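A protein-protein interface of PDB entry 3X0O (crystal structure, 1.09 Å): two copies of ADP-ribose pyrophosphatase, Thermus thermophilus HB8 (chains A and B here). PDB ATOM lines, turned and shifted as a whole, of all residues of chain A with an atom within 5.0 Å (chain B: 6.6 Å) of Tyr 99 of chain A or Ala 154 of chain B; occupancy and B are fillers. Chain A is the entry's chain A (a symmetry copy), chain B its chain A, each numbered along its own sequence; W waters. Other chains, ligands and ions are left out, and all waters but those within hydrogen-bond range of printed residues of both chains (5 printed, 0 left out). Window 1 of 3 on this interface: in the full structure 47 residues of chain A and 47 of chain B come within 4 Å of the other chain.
Phe 97 of chain A touches His 145 of chain B.
Phe 97 of chain A touches Leu 157 of chain B.
OG of Ser 98 of chain A touches OE1 of Glu 151 of chain B, at 3.9 Å.
O of Ser 98 of chain A touches CB of Phe 152 of chain B, 3.8 Å away.
Ser 153 of chain B touches Tyr 99 of chain A.
Ala 154 of chain B touches Tyr 99 of chain A (CB to CD2, 3.6 Å).
Tyr 99 of chain A touches Leu 157 of chain B.
Ser 153 of chain B touches Phe 100 of chain A.
CB of Ala 154 of chain B touches O of Val 101 of chain A (3.7 Å).
Ala 154 of chain A touches Val 101 of chain B (CB to O, 3.7 Å).
N of Leu 62 of chain B is in hydrogen-bond range of O of Glu 151 of chain B (2.8 Å).
The side-chain hydroxyl (OG) of Ser 153 of chain B is in hydrogen-bond range of the side-chain hydroxyl (OG1) of Thr 155 of chain B, 2.9 Å away.
N of Gly 156 of chain B is in hydrogen-bond range of OG of Ser 153 of chain B (3.1 Å).
The backbone carbonyl oxygen (O) of Phe 97 of chain A is in hydrogen-bond range of the backbone NH (N) of Val 112 of chain A (2.8 Å).
The backbone NH (N) of Thr 110 of chain A sits at hydrogen-bond distance from the backbone carbonyl oxygen (O) of Tyr 99 of chain A (2.8 Å).
N of Val 101 of chain A is in hydrogen-bond range of O of Glu 108 of chain A (3.1 Å).
Tyr 99 of chain A touches Ala 154 of chain B, and with the chains exchanged Ala 154 of chain A touches Tyr 99 of chain B.
Val 101 of chain A touches its own counterpart, Val 101 of chain B.
Val 101 of chain A touches Ala 154 of chain B, and with the chains exchanged Ala 154 of chain A touches Val 101 of chain B.
Positions printed for both chains: 99, 101, 154, 155 and 158.
Of the 14 printed residues of chain B, 8 touch a printed residue of chain A.
Printed residues of chain B that touch a printed residue of chain A: Tyr 99, Val 101, His 145, Glu 151, Phe 152, Ser 153, Ala 154 and Leu 157.
Along chain B the printed residues that touch a printed residue of chain A span positions 99 to 157.
Printed residues of chain A that touch a printed residue of chain B: Phe 97, Ser 98, Tyr 99, Phe 100, Val 101, Lys 109 and Ala 154.
N of Ser 98 of chain A is in hydrogen-bond range of NE2 of His 145 of chain B.
The side-chain carboxylate (OE1) of Glu 151 of chain B lies within salt-bridge range of the side-chain amino group (NZ) of Lys 109 of chain A (3.0 Å).
The backbone NH of Phe 100 of chain A sits at hydrogen-bond distance from the backbone carbonyl oxygen of Phe 152 of chain B (2.8 Å).
N of Ala 154 of chain B sits at hydrogen-bond distance from O of Phe 100 of chain A (2.8 Å).
Of the printed residues of chain A, His 145 of chain B touches Phe 97 (3.4 Å) and Ser 98 (3.1 Å).
Of the printed residues of chain A, Phe 152 of chain B touches Ser 98 (3.8 Å), Tyr 99 (3.3 Å) and Phe 100 (2.8 Å).
Of the printed residues of chain A, Ala 154 of chain B touches Tyr 99 (3.6 Å), Phe 100 (2.8 Å) and Val 101 (3.7 Å).
Gly 159 of chain B touches none of the printed residues of chain A.
The nearest residue of chain B that does not touch Tyr 99 of chain A is Val 101 of chain B (5.2 Å).
The nearest residue of chain A that does not touch Ala 154 of chain B is Ala 154 of chain A (4.9 Å).
The nearest printed residue of chain A that does not touch His 145 of chain B is Tyr 99 of chain A (5.3 Å).
Water W2 lies within hydrogen-bond range of OE1 of Glu 151 of chain B (2.7 Å), N of Phe 152 of chain B (2.9 Å) and OG of Ser 98 of chain A (3.0 Å).
Water W3 lies within hydrogen-bond range of the side-chain hydroxyl of Ser 98 of chain A, the side-chain amino group of Lys 109 of chain A and the side-chain carboxylate of Glu 151 of chain B.
Water W4 lies within hydrogen-bond range of the backbone carbonyl oxygen of Val 101 of chain B and the side-chain hydroxyl of Tyr 99 of chain A.
Water W1 bridges the backbone carbonyl oxygen (O) of Val 101 of chain A (2.8 Å) and the side-chain hydroxyl (OH) of Tyr 99 of chain B (2.8 Å).
Water W5 lies within hydrogen-bond range of O of Val 101 of chain B and O of Val 101 of chain A.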
ATOM      1  N   PHE A  97      19.804  -0.719  28.580  1.00  0.00           N
ATOM      2  CA  PHE A  97      18.894   0.357  28.172  1.00  0.00           C
ATOM      3  C   PHE A  97      19.537   1.110  27.007  1.00  0.00           C
ATOM      4  O   PHE A  97      20.708   0.845  26.651  1.00  0.00           O
ATOM      5  CB  PHE A  97      18.565   1.313  29.333  1.00  0.00           C
ATOM      6  CG  PHE A  97      19.729   1.657  30.258  1.00  0.00           C
ATOM      7  CD1 PHE A  97      19.603   1.357  31.618  1.00  0.00           C
ATOM      8  CD2 PHE A  97      20.894   2.300  29.776  1.00  0.00           C
ATOM      9  CE1 PHE A  97      20.643   1.674  32.476  1.00  0.00           C
ATOM     10  CE2 PHE A  97      21.953   2.564  30.617  1.00  0.00           C
ATOM     11  CZ  PHE A  97      21.844   2.206  31.997  1.00  0.00           C
ATOM     12  N   SER A  98      18.776   1.987  26.399  1.00  0.00           N
ATOM     13  CA  SER A  98      19.244   2.789  25.275  1.00  0.00           C
ATOM     14  C   SER A  98      18.877   4.226  25.499  1.00  0.00           C
ATOM     15  O   SER A  98      17.988   4.535  26.291  1.00  0.00           O
ATOM     16  CB  SER A  98      18.601   2.307  23.976  1.00  0.00           C
ATOM     17  OG  SER A  98      17.212   2.553  24.058  1.00  0.00           O
ATOM     18  N   TYR A  99      19.547   5.103  24.754  1.00  0.00           N
ATOM     19  CA  TYR A  99      19.161   6.528  24.809  1.00  0.00           C
ATOM     20  C   TYR A  99      19.535   7.222  23.500  1.00  0.00           C
ATOM     21  O   TYR A  99      20.498   6.836  22.825  1.00  0.00           O
ATOM     22  CB  TYR A  99      19.804   7.266  25.996  1.00  0.00           C
ATOM     23  CG  TYR A  99      21.344   7.341  25.915  1.00  0.00           C
ATOM     24  CD1 TYR A  99      22.134   6.278  26.411  1.00  0.00           C
ATOM     25  CD2 TYR A  99      21.976   8.440  25.363  1.00  0.00           C
ATOM     26  CE1 TYR A  99      23.551   6.359  26.330  1.00  0.00           C
ATOM     27  CE2 TYR A  99      23.351   8.525  25.299  1.00  0.00           C
ATOM     28  CZ  TYR A  99      24.156   7.479  25.788  1.00  0.00           C
ATOM     29  OH  TYR A  99      25.507   7.512  25.730  1.00  0.00           O
ATOM     30  N   PHE A 100      18.755   8.232  23.181  1.00  0.00           N
ATOM     31  CA  PHE A 100      19.125   9.159  22.110  1.00  0.00           C
ATOM     32  C   PHE A 100      20.078  10.201  22.627  1.00  0.00           C
ATOM     33  O   PHE A 100      19.762  10.888  23.613  1.00  0.00           O
ATOM     34  CB  PHE A 100      17.854   9.843  21.530  1.00  0.00           C
ATOM     35  CG  PHE A 100      17.013   8.882  20.751  1.00  0.00           C
ATOM     36  CD1 PHE A 100      15.776   8.435  21.242  1.00  0.00           C
ATOM     37  CD2 PHE A 100      17.415   8.427  19.512  1.00  0.00           C
ATOM     38  CE1 PHE A 100      14.951   7.552  20.499  1.00  0.00           C
ATOM     39  CE2 PHE A 100      16.608   7.570  18.754  1.00  0.00           C
ATOM     40  CZ  PHE A 100      15.404   7.165  19.243  1.00  0.00           C
ATOM     41  N   VAL A 101      21.257  10.340  21.984  1.00  0.00           N
ATOM     42  CA  VAL A 101      22.301  11.189  22.547  1.00  0.00           C
ATOM     43  C   VAL A 101      21.881  12.656  22.621  1.00  0.00           C
ATOM     44  O   VAL A 101      22.324  13.355  23.533  1.00  0.00           O
ATOM     45  CB  VAL A 101      23.650  11.090  21.759  1.00  0.00           C
ATOM     46  CG1 VAL A 101      24.027   9.598  21.624  1.00  0.00           C
ATOM     47  CG2 VAL A 101      23.642  11.788  20.435  1.00  0.00           C
ATOM     48  N   GLU A 108      21.180   9.797  16.525  1.00  0.00           N
ATOM     49  CA  GLU A 108      22.076   8.790  17.076  1.00  0.00           C
ATOM     50  C   GLU A 108      21.462   8.179  18.357  1.00  0.00           C
ATOM     51  O   GLU A 108      21.112   8.897  19.287  1.00  0.00           O
ATOM     52  CB  GLU A 108      23.440   9.364  17.399  1.00  0.00           C
ATOM     53  CG  GLU A 108      24.424   8.290  17.897  1.00  0.00           C
ATOM     54  CD  GLU A 108      25.759   8.864  18.316  1.00  0.00           C
ATOM     55  OE1 GLU A 108      25.961  10.030  18.559  1.00  0.00           O
ATOM     56  OE2 GLU A 108      26.727   7.967  18.339  1.00  0.00           O
ATOM     57  N   LYS A 109      21.422   6.861  18.381  1.00  0.00           N
ATOM     58  CA  LYS A 109      20.899   6.099  19.507  1.00  0.00           C
ATOM     59  C   LYS A 109      22.037   5.201  20.030  1.00  0.00           C
ATOM     60  O   LYS A 109      22.718   4.582  19.195  1.00  0.00           O
ATOM     61  CB  LYS A 109      19.700   5.270  19.071  1.00  0.00           C
ATOM     62  CG  LYS A 109      18.981   4.587  20.226  1.00  0.00           C
ATOM     63  CD  LYS A 109      17.748   3.793  19.662  1.00  0.00           C
ATOM     64  CE  LYS A 109      16.716   3.576  20.809  1.00  0.00           C
ATOM     65  NZ  LYS A 109      15.607   2.654  20.310  1.00  0.00           N
ATOM     66  N   THR A 110      22.202   5.156  21.336  1.00  0.00           N
ATOM     67  CA  THR A 110      23.199   4.346  21.983  1.00  0.00           C
ATOM     68  C   THR A 110      22.559   3.242  22.796  1.00  0.00           C
ATOM     69  O   THR A 110      21.689   3.521  23.605  1.00  0.00           O
ATOM     70  CB  THR A 110      24.063   5.220  22.901  1.00  0.00           C
ATOM     71  OG1 THR A 110      24.659   6.279  22.126  1.00  0.00           O
ATOM     72  CG2 THR A 110      25.219   4.477  23.524  1.00  0.00           C
ATOM     73  N   VAL A 112      23.262   0.402  25.578  1.00  0.00           N
ATOM     74  CA  VAL A 112      24.231   0.222  26.656  1.00  0.00           C
ATOM     75  C   VAL A 112      24.112  -1.194  27.236  1.00  0.00           C
ATOM     76  O   VAL A 112      22.994  -1.671  27.530  1.00  0.00           O
ATOM     77  CB  VAL A 112      23.994   1.272  27.773  1.00  0.00           C
ATOM     78  CG1 VAL A 112      25.111   1.154  28.828  1.00  0.00           C
ATOM     79  CG2 VAL A 112      23.958   2.673  27.192  1.00  0.00           C
ATOM     80  N   ALA A 154      28.863  11.362  27.489  1.00  0.00           N
ATOM     81  CA  ALA A 154      27.606  10.792  28.014  1.00  0.00           C
ATOM     82  C   ALA A 154      27.828   9.350  28.434  1.00  0.00           C
ATOM     83  O   ALA A 154      27.303   8.916  29.465  1.00  0.00           O
ATOM     84  CB  ALA A 154      26.514  10.871  26.952  1.00  0.00           C
ATOM     85  N   THR A 155      28.554   8.563  27.629  1.00  0.00           N
ATOM     86  CA  THR A 155      28.696   7.139  28.013  1.00  0.00           C
ATOM     87  C   THR A 155      29.476   7.021  29.317  1.00  0.00           C
ATOM     88  O   THR A 155      29.113   6.160  30.162  1.00  0.00           O
ATOM     89  CB  THR A 155      29.365   6.324  26.913  1.00  0.00           C
ATOM     90  OG1 THR A 155      30.696   6.816  26.639  1.00  0.00           O
ATOM     91  CG2 THR A 155      28.559   6.312  25.593  1.00  0.00           C
ATOM     92  N   VAL A 158      27.069   8.042  32.155  1.00  0.00           N
ATOM     93  CA  VAL A 158      26.051   6.965  32.349  1.00  0.00           C
ATOM     94  C   VAL A 158      26.682   5.798  33.094  1.00  0.00           C
ATOM     95  O   VAL A 158      26.060   5.245  34.007  1.00  0.00           O
ATOM     96  CB  VAL A 158      25.479   6.573  30.983  1.00  0.00           C
ATOM     97  CG1 VAL A 158      24.762   5.212  31.044  1.00  0.00           C
ATOM     98  CG2 VAL A 158      24.537   7.684  30.468  1.00  0.00           C
ATOM     99  N   LEU B  62      11.394  10.508  26.349  1.00  0.00           N
ATOM    100  CA  LEU B  62      11.300  11.081  27.720  1.00  0.00           C
ATOM    101  C   LEU B  62      12.582  11.827  27.999  1.00  0.00           C
ATOM    102  O   LEU B  62      13.693  11.202  28.016  1.00  0.00           O
ATOM    103  CB  LEU B  62      11.084   9.958  28.695  1.00  0.00           C
ATOM    104  CG  LEU B  62      10.479  10.377  30.007  1.00  0.00           C
ATOM    105  CD1 LEU B  62       9.004  10.800  29.849  1.00  0.00           C
ATOM    106  CD2 LEU B  62      10.585   9.197  31.007  1.00  0.00           C
ATOM    107  N   ILE B  64      14.354  15.372  30.368  1.00  0.00           N
ATOM    108  CA  ILE B  64      14.131  16.321  31.462  1.00  0.00           C
ATOM    109  C   ILE B  64      14.194  17.707  30.851  1.00  0.00           C
ATOM    110  O   ILE B  64      14.686  17.881  29.729  1.00  0.00           O
ATOM    111  CB  ILE B  64      15.114  16.101  32.643  1.00  0.00           C
ATOM    112  CG1 ILE B  64      16.544  16.168  32.155  1.00  0.00           C
ATOM    113  CG2 ILE B  64      14.794  14.789  33.371  1.00  0.00           C
ATOM    114  CD1 ILE B  64      17.598  16.055  33.283  1.00  0.00           C
ATOM    115  N   TYR B  99      28.530  16.864  30.559  1.00  0.00           N
ATOM    116  CA  TYR B  99      29.007  15.775  29.681  1.00  0.00           C
ATOM    117  C   TYR B  99      28.939  16.216  28.219  1.00  0.00           C
ATOM    118  O   TYR B  99      28.093  17.034  27.837  1.00  0.00           O
ATOM    119  CB  TYR B  99      28.212  14.473  29.873  1.00  0.00           C
ATOM    120  CG  TYR B  99      26.725  14.594  29.478  1.00  0.00           C
ATOM    121  CD1 TYR B  99      25.777  15.071  30.412  1.00  0.00           C
ATOM    122  CD2 TYR B  99      26.293  14.237  28.212  1.00  0.00           C
ATOM    123  CE1 TYR B  99      24.411  15.178  30.035  1.00  0.00           C
ATOM    124  CE2 TYR B  99      24.965  14.327  27.852  1.00  0.00           C
ATOM    125  CZ  TYR B  99      24.005  14.799  28.767  1.00  0.00           C
ATOM    126  OH  TYR B  99      22.695  14.918  28.451  1.00  0.00           O
ATOM    127  N   VAL B 101      27.774  15.167  24.679  1.00  0.00           N
ATOM    128  CA  VAL B 101      26.712  14.248  24.287  1.00  0.00           C
ATOM    129  C   VAL B 101      27.222  13.115  23.399  1.00  0.00           C
ATOM    130  O   VAL B 101      26.671  12.014  23.465  1.00  0.00           O
ATOM    131  CB  VAL B 101      25.530  14.969  23.555  1.00  0.00           C
ATOM    132  CG1 VAL B 101      25.073  16.160  24.425  1.00  0.00           C
ATOM    133  CG2 VAL B 101      25.840  15.388  22.151  1.00  0.00           C
ATOM    134  N   HIS B 145      10.548   2.127  30.092  1.00  0.00           N
ATOM    135  CA  HIS B 145      11.604   1.979  29.103  1.00  0.00           C
ATOM    136  C   HIS B 145      12.021   0.524  28.916  1.00  0.00           C
ATOM    137  O   HIS B 145      12.205   0.065  27.784  1.00  0.00           O
ATOM    138  CB  HIS B 145      12.805   2.859  29.565  1.00  0.00           C
ATOM    139  CG  HIS B 145      13.950   2.720  28.540  1.00  0.00           C
ATOM    140  ND1 HIS B 145      13.891   3.235  27.270  1.00  0.00           N
ATOM    141  CD2 HIS B 145      15.140   2.080  28.638  1.00  0.00           C
ATOM    142  CE1 HIS B 145      15.052   2.938  26.643  1.00  0.00           C
ATOM    143  NE2 HIS B 145      15.839   2.200  27.423  1.00  0.00           N
ATOM    144  N   GLU B 151      11.053   5.826  24.918  1.00  0.00           N
ATOM    145  CA  GLU B 151      12.491   5.974  24.628  1.00  0.00           C
ATOM    146  C   GLU B 151      13.017   7.064  25.555  1.00  0.00           C
ATOM    147  O   GLU B 151      12.251   7.869  26.037  1.00  0.00           O
ATOM    148  CB  GLU B 151      12.727   6.382  23.197  1.00  0.00           C
ATOM    149  CG  GLU B 151      12.131   5.408  22.158  1.00  0.00           C
ATOM    150  CD  GLU B 151      12.737   4.046  22.288  1.00  0.00           C
ATOM    151  OE1 GLU B 151      13.959   3.936  22.518  1.00  0.00           O
ATOM    152  OE2 GLU B 151      12.029   3.025  22.204  1.00  0.00           O
ATOM    153  N   PHE B 152      14.325   7.029  25.842  1.00  0.00           N
ATOM    154  CA  PHE B 152      14.951   8.065  26.636  1.00  0.00           C
ATOM    155  C   PHE B 152      15.808   8.949  25.766  1.00  0.00           C
ATOM    156  O   PHE B 152      16.459   8.476  24.839  1.00  0.00           O
ATOM    157  CB  PHE B 152      15.942   7.457  27.657  1.00  0.00           C
ATOM    158  CG  PHE B 152      15.347   6.970  28.940  1.00  0.00           C
ATOM    159  CD1 PHE B 152      15.588   5.671  29.388  1.00  0.00           C
ATOM    160  CD2 PHE B 152      14.624   7.808  29.745  1.00  0.00           C
ATOM    161  CE1 PHE B 152      15.091   5.198  30.600  1.00  0.00           C
ATOM    162  CE2 PHE B 152      14.108   7.342  30.935  1.00  0.00           C
ATOM    163  CZ  PHE B 152      14.326   6.043  31.376  1.00  0.00           C
ATOM    164  N   SER B 153      15.874  10.233  26.143  1.00  0.00           N
ATOM    165  CA  SER B 153      17.035  11.019  25.710  1.00  0.00           C
ATOM    166  C   SER B 153      18.164  10.757  26.732  1.00  0.00           C
ATOM    167  O   SER B 153      17.921  10.281  27.839  1.00  0.00           O
ATOM    168  CB  SER B 153      16.730  12.507  25.643  1.00  0.00           C
ATOM    169  OG  SER B 153      16.464  12.977  26.993  1.00  0.00           O
ATOM    170  N   ALA B 154      19.374  11.198  26.374  1.00  0.00           N
ATOM    171  CA  ALA B 154      20.463  11.145  27.371  1.00  0.00           C
ATOM    172  C   ALA B 154      20.057  11.904  28.621  1.00  0.00           C
ATOM    173  O   ALA B 154      20.345  11.459  29.738  1.00  0.00           O
ATOM    174  CB  ALA B 154      21.737  11.743  26.781  1.00  0.00           C
ATOM    175  N   THR B 155      19.437  13.082  28.472  1.00  0.00           N
ATOM    176  CA  THR B 155      19.116  13.845  29.700  1.00  0.00           C
ATOM    177  C   THR B 155      18.099  13.085  30.543  1.00  0.00           C
ATOM    178  O   THR B 155      18.231  13.087  31.796  1.00  0.00           O
ATOM    179  CB  THR B 155      18.604  15.243  29.375  1.00  0.00           C
ATOM    180  OG1 THR B 155      17.390  15.183  28.594  1.00  0.00           O
ATOM    181  CG2 THR B 155      19.640  16.106  28.617  1.00  0.00           C
ATOM    182  N   GLY B 156      17.097  12.443  29.936  1.00  0.00           N
ATOM    183  CA  GLY B 156      16.137  11.665  30.728  1.00  0.00           C
ATOM    184  C   GLY B 156      16.801  10.508  31.462  1.00  0.00           C
ATOM    185  O   GLY B 156      16.516  10.257  32.632  1.00  0.00           O
ATOM    186  N   LEU B 157      17.682   9.783  30.744  1.00  0.00           N
ATOM    187  CA  LEU B 157      18.366   8.664  31.363  1.00  0.00           C
ATOM    188  C   LEU B 157      19.270   9.122  32.481  1.00  0.00           C
ATOM    189  O   LEU B 157      19.308   8.510  33.566  1.00  0.00           O
ATOM    190  CB  LEU B 157      19.160   7.895  30.294  1.00  0.00           C
ATOM    191  CG  LEU B 157      19.981   6.733  30.842  1.00  0.00           C
ATOM    192  CD1 LEU B 157      19.105   5.658  31.501  1.00  0.00           C
ATOM    193  CD2 LEU B 157      20.805   6.147  29.689  1.00  0.00           C
ATOM    194  N   VAL B 158      20.004  10.200  32.259  1.00  0.00           N
ATOM    195  CA  VAL B 158      20.881  10.759  33.331  1.00  0.00           C
ATOM    196  C   VAL B 158      20.035  11.125  34.541  1.00  0.00           C
ATOM    197  O   VAL B 158      20.430  10.841  35.676  1.00  0.00           O
ATOM    198  CB  VAL B 158      21.668  11.944  32.760  1.00  0.00           C
ATOM    199  CG1 VAL B 158      22.255  12.821  33.882  1.00  0.00           C
ATOM    200  CG2 VAL B 158      22.771  11.433  31.807  1.00  0.00           C
ATOM    201  N   GLY B 159      18.850  11.760  34.320  1.00  0.00           N
ATOM    202  CA  GLY B 159      18.016  12.092  35.482  1.00  0.00           C
ATOM    203  C   GLY B 159      17.605  10.842  36.253  1.00  0.00           C
ATOM    204  O   GLY B 159      17.652  10.780  37.481  1.00  0.00           O
HETATM  205  O   HOH W   1      21.913  15.058  25.729  1.00  0.00           O
HETATM  206  O   HOH W   2      15.689   5.086  24.164  1.00  0.00           O
HETATM  207  O   HOH W   3      15.328   0.954  22.784  1.00  0.00           O
HETATM  208  O   HOH W   4      26.793   9.241  23.886  1.00  0.00           O
HETATM  209  O   HOH W   5      24.314  12.005  25.162  1.00  0.00           O
